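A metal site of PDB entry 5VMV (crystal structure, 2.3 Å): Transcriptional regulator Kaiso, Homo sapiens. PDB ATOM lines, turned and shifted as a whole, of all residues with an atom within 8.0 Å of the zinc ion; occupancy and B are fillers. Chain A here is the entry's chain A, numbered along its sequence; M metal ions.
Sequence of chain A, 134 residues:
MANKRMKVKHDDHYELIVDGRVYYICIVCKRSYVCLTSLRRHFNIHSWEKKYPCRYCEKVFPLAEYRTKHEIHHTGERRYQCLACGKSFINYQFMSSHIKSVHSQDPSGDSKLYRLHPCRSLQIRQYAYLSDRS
Within 4 Å of the zinc ion: Cys 82, Cys 85, His 98 and His 103.
The backbone NH (N) of Ala 84 lies close to the side-chain sulfur (SG) of Cys 82 (3.2 Å).
The backbone carbonyl oxygen (O) of Lys 87 lies within hydrogen-bond range of the backbone NH (N) of Cys 82, 2.9 Å away.
The side-chain sulfur (SG) of Cys 85 lies close to the backbone NH (N) of Lys 87.
The zinc ion is bound by NE2 of His 98 (1.9 Å), NE2 of His 103 (2.0 Å), SG of Cys 82 (2.3 Å) and SG of Cys 85 (2.3 Å).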
ATOM      1  N   GLN A  81     -10.509 -24.843  21.060  1.00  0.00           N
ATOM      2  CA  GLN A  81     -11.554 -23.808  20.923  1.00  0.00           C
ATOM      3  C   GLN A  81     -12.673 -24.238  20.000  1.00  0.00           C
ATOM      4  O   GLN A  81     -12.422 -24.686  18.872  1.00  0.00           O
ATOM      5  CB  GLN A  81     -10.957 -22.475  20.411  1.00  0.00           C
ATOM      6  CG  GLN A  81     -11.974 -21.285  20.389  1.00  0.00           C
ATOM      7  CD  GLN A  81     -11.313 -19.974  19.999  1.00  0.00           C
ATOM      8  OE1 GLN A  81     -10.273 -19.958  19.319  1.00  0.00           O
ATOM      9  NE2 GLN A  81     -11.906 -18.863  20.425  1.00  0.00           N
ATOM     10  N   CYS A  82     -13.919 -24.129  20.496  1.00  0.00           N
ATOM     11  CA  CYS A  82     -15.102 -24.369  19.687  1.00  0.00           C
ATOM     12  C   CYS A  82     -15.217 -23.236  18.687  1.00  0.00           C
ATOM     13  O   CYS A  82     -15.088 -22.065  19.078  1.00  0.00           O
ATOM     14  CB  CYS A  82     -16.362 -24.435  20.558  1.00  0.00           C
ATOM     15  SG  CYS A  82     -17.891 -24.249  19.636  1.00  0.00           S
ATOM     16  N   LEU A  83     -15.477 -23.540  17.424  1.00  0.00           N
ATOM     17  CA  LEU A  83     -15.468 -22.503  16.394  1.00  0.00           C
ATOM     18  C   LEU A  83     -16.872 -22.009  16.171  1.00  0.00           C
ATOM     19  O   LEU A  83     -17.093 -21.057  15.418  1.00  0.00           O
ATOM     20  CB  LEU A  83     -14.859 -23.005  15.081  1.00  0.00           C
ATOM     21  CG  LEU A  83     -13.353 -23.298  15.162  1.00  0.00           C
ATOM     22  CD1 LEU A  83     -12.749 -23.729  13.798  1.00  0.00           C
ATOM     23  CD2 LEU A  83     -12.640 -22.092  15.700  1.00  0.00           C
ATOM     24  N   ALA A  84     -17.827 -22.628  16.856  1.00  0.00           N
ATOM     25  CA  ALA A  84     -19.210 -22.223  16.719  1.00  0.00           C
ATOM     26  C   ALA A  84     -19.585 -21.068  17.630  1.00  0.00           C
ATOM     27  O   ALA A  84     -20.469 -20.274  17.285  1.00  0.00           O
ATOM     28  CB  ALA A  84     -20.130 -23.426  16.994  1.00  0.00           C
ATOM     29  N   CYS A  85     -18.932 -20.954  18.792  1.00  0.00           N
ATOM     30  CA  CYS A  85     -19.245 -19.885  19.755  1.00  0.00           C
ATOM     31  C   CYS A  85     -17.983 -19.304  20.414  1.00  0.00           C
ATOM     32  O   CYS A  85     -18.055 -18.283  21.088  1.00  0.00           O
ATOM     33  CB  CYS A  85     -20.169 -20.413  20.840  1.00  0.00           C
ATOM     34  SG  CYS A  85     -19.305 -21.574  21.960  1.00  0.00           S
ATOM     35  N   GLY A  86     -16.832 -19.958  20.250  1.00  0.00           N
ATOM     36  CA  GLY A  86     -15.553 -19.371  20.624  1.00  0.00           C
ATOM     37  C   GLY A  86     -15.012 -19.817  21.971  1.00  0.00           C
ATOM     38  O   GLY A  86     -13.889 -19.467  22.342  1.00  0.00           O
ATOM     39  N   LYS A  87     -15.798 -20.603  22.694  1.00  0.00           N
ATOM     40  CA  LYS A  87     -15.394 -21.041  24.038  1.00  0.00           C
ATOM     41  C   LYS A  87     -14.197 -21.975  23.982  1.00  0.00           C
ATOM     42  O   LYS A  87     -14.109 -22.822  23.105  1.00  0.00           O
ATOM     43  CB  LYS A  87     -16.548 -21.754  24.735  1.00  0.00           C
ATOM     44  CG  LYS A  87     -17.649 -20.824  25.244  1.00  0.00           C
ATOM     45  CD  LYS A  87     -18.299 -21.455  26.443  1.00  0.00           C
ATOM     46  CE  LYS A  87     -19.789 -21.597  26.262  1.00  0.00           C
ATOM     47  NZ  LYS A  87     -20.458 -20.288  26.378  1.00  0.00           N
ATOM     48  N   SER A  88     -13.274 -21.838  24.936  1.00  0.00           N
ATOM     49  CA  SER A  88     -12.080 -22.668  24.956  1.00  0.00           C
ATOM     50  C   SER A  88     -12.110 -23.764  26.046  1.00  0.00           C
ATOM     51  O   SER A  88     -12.812 -23.625  27.048  1.00  0.00           O
ATOM     52  CB  SER A  88     -10.863 -21.784  25.109  1.00  0.00           C
ATOM     53  OG  SER A  88     -10.791 -20.895  24.012  1.00  0.00           O
ATOM     54  N   PHE A  89     -11.337 -24.841  25.838  1.00  0.00           N
ATOM     55  CA  PHE A  89     -11.345 -26.013  26.743  1.00  0.00           C
ATOM     56  C   PHE A  89      -9.957 -26.615  26.820  1.00  0.00           C
ATOM     57  O   PHE A  89      -9.127 -26.475  25.900  1.00  0.00           O
ATOM     58  CB  PHE A  89     -12.357 -27.072  26.278  1.00  0.00           C
ATOM     59  CG  PHE A  89     -13.735 -26.518  26.067  1.00  0.00           C
ATOM     60  CD1 PHE A  89     -14.658 -26.490  27.112  1.00  0.00           C
ATOM     61  CD2 PHE A  89     -14.087 -25.971  24.858  1.00  0.00           C
ATOM     62  CE1 PHE A  89     -15.935 -25.936  26.941  1.00  0.00           C
ATOM     63  CE2 PHE A  89     -15.372 -25.440  24.674  1.00  0.00           C
ATOM     64  CZ  PHE A  89     -16.278 -25.417  25.732  1.00  0.00           C
ATOM     65  N   MET A  95     -14.135 -30.304  24.881  1.00  0.00           N
ATOM     66  CA  MET A  95     -14.492 -29.602  23.655  1.00  0.00           C
ATOM     67  C   MET A  95     -15.571 -30.428  22.949  1.00  0.00           C
ATOM     68  O   MET A  95     -16.628 -29.909  22.618  1.00  0.00           O
ATOM     69  CB  MET A  95     -13.250 -29.394  22.755  1.00  0.00           C
ATOM     70  CG  MET A  95     -13.563 -28.949  21.303  1.00  0.00           C
ATOM     71  SD  MET A  95     -14.199 -30.252  20.214  1.00  0.00           S
ATOM     72  CE  MET A  95     -12.783 -31.358  20.093  1.00  0.00           C
ATOM     73  N   HIS A  98     -18.788 -30.434  24.740  1.00  0.00           N
ATOM     74  CA  HIS A  98     -19.409 -29.118  24.518  1.00  0.00           C
ATOM     75  C   HIS A  98     -20.134 -29.054  23.188  1.00  0.00           C
ATOM     76  O   HIS A  98     -21.312 -28.732  23.128  1.00  0.00           O
ATOM     77  CB  HIS A  98     -18.385 -27.989  24.541  1.00  0.00           C
ATOM     78  CG  HIS A  98     -18.905 -26.723  23.956  1.00  0.00           C
ATOM     79  ND1 HIS A  98     -19.748 -25.871  24.651  1.00  0.00           N
ATOM     80  CD2 HIS A  98     -18.689 -26.134  22.754  1.00  0.00           C
ATOM     81  CE1 HIS A  98     -20.069 -24.845  23.876  1.00  0.00           C
ATOM     82  NE2 HIS A  98     -19.431 -24.963  22.737  1.00  0.00           N
ATOM     83  N   ILE A  99     -19.412 -29.344  22.124  1.00  0.00           N
ATOM     84  CA  ILE A  99     -19.994 -29.183  20.815  1.00  0.00           C
ATOM     85  C   ILE A  99     -21.177 -30.119  20.610  1.00  0.00           C
ATOM     86  O   ILE A  99     -22.227 -29.691  20.132  1.00  0.00           O
ATOM     87  CB  ILE A  99     -18.938 -29.400  19.762  1.00  0.00           C
ATOM     88  CG1 ILE A  99     -17.886 -28.316  19.926  1.00  0.00           C
ATOM     89  CG2 ILE A  99     -19.537 -29.328  18.365  1.00  0.00           C
ATOM     90  CD1 ILE A  99     -16.946 -28.181  18.741  1.00  0.00           C
ATOM     91  N   LYS A 100     -21.026 -31.385  20.993  1.00  0.00           N
ATOM     92  CA  LYS A 100     -22.155 -32.315  20.833  1.00  0.00           C
ATOM     93  C   LYS A 100     -23.366 -31.830  21.609  1.00  0.00           C
ATOM     94  O   LYS A 100     -24.487 -31.801  21.102  1.00  0.00           O
ATOM     95  CB  LYS A 100     -21.773 -33.728  21.283  1.00  0.00           C
ATOM     96  CG  LYS A 100     -20.866 -34.485  20.312  1.00  0.00           C
ATOM     97  CD  LYS A 100     -20.497 -35.882  20.834  1.00  0.00           C
ATOM     98  CE  LYS A 100     -19.676 -36.686  19.821  1.00  0.00           C
ATOM     99  NZ  LYS A 100     -19.237 -38.020  20.350  1.00  0.00           N
ATOM    100  N   VAL A 102     -24.150 -28.679  23.124  1.00  0.00           N
ATOM    101  CA  VAL A 102     -24.617 -27.316  22.959  1.00  0.00           C
ATOM    102  C   VAL A 102     -24.986 -27.045  21.509  1.00  0.00           C
ATOM    103  O   VAL A 102     -25.961 -26.364  21.245  1.00  0.00           O
ATOM    104  CB  VAL A 102     -23.530 -26.264  23.389  1.00  0.00           C
ATOM    105  CG1 VAL A 102     -23.951 -24.811  22.984  1.00  0.00           C
ATOM    106  CG2 VAL A 102     -23.240 -26.319  24.885  1.00  0.00           C
ATOM    107  N   HIS A 103     -24.194 -27.587  20.592  1.00  0.00           N
ATOM    108  CA  HIS A 103     -24.307 -27.340  19.170  1.00  0.00           C
ATOM    109  C   HIS A 103     -24.882 -28.522  18.357  1.00  0.00           C
ATOM    110  O   HIS A 103     -24.906 -28.458  17.115  1.00  0.00           O
ATOM    111  CB  HIS A 103     -22.931 -26.957  18.617  1.00  0.00           C
ATOM    112  CG  HIS A 103     -22.351 -25.731  19.237  1.00  0.00           C
ATOM    113  ND1 HIS A 103     -22.963 -24.497  19.158  1.00  0.00           N
ATOM    114  CD2 HIS A 103     -21.191 -25.528  19.913  1.00  0.00           C
ATOM    115  CE1 HIS A 103     -22.227 -23.599  19.778  1.00  0.00           C
ATOM    116  NE2 HIS A 103     -21.144 -24.184  20.243  1.00  0.00           N
ATOM    117  N   LEU A 113     -14.919 -28.085  13.260  1.00  0.00           N
ATOM    118  CA  LEU A 113     -15.784 -27.536  14.303  1.00  0.00           C
ATOM    119  C   LEU A 113     -14.942 -26.996  15.490  1.00  0.00           C
ATOM    120  O   LEU A 113     -15.444 -26.258  16.349  1.00  0.00           O
ATOM    121  CB  LEU A 113     -16.791 -28.589  14.796  1.00  0.00           C
ATOM    122  CG  LEU A 113     -17.844 -29.091  13.776  1.00  0.00           C
ATOM    123  CD1 LEU A 113     -18.858 -30.063  14.388  1.00  0.00           C
ATOM    124  CD2 LEU A 113     -18.562 -27.950  13.119  1.00  0.00           C
HETATM  125 ZN    ZN M   1     -19.430 -23.757  21.236  1.00  0.00          ZN
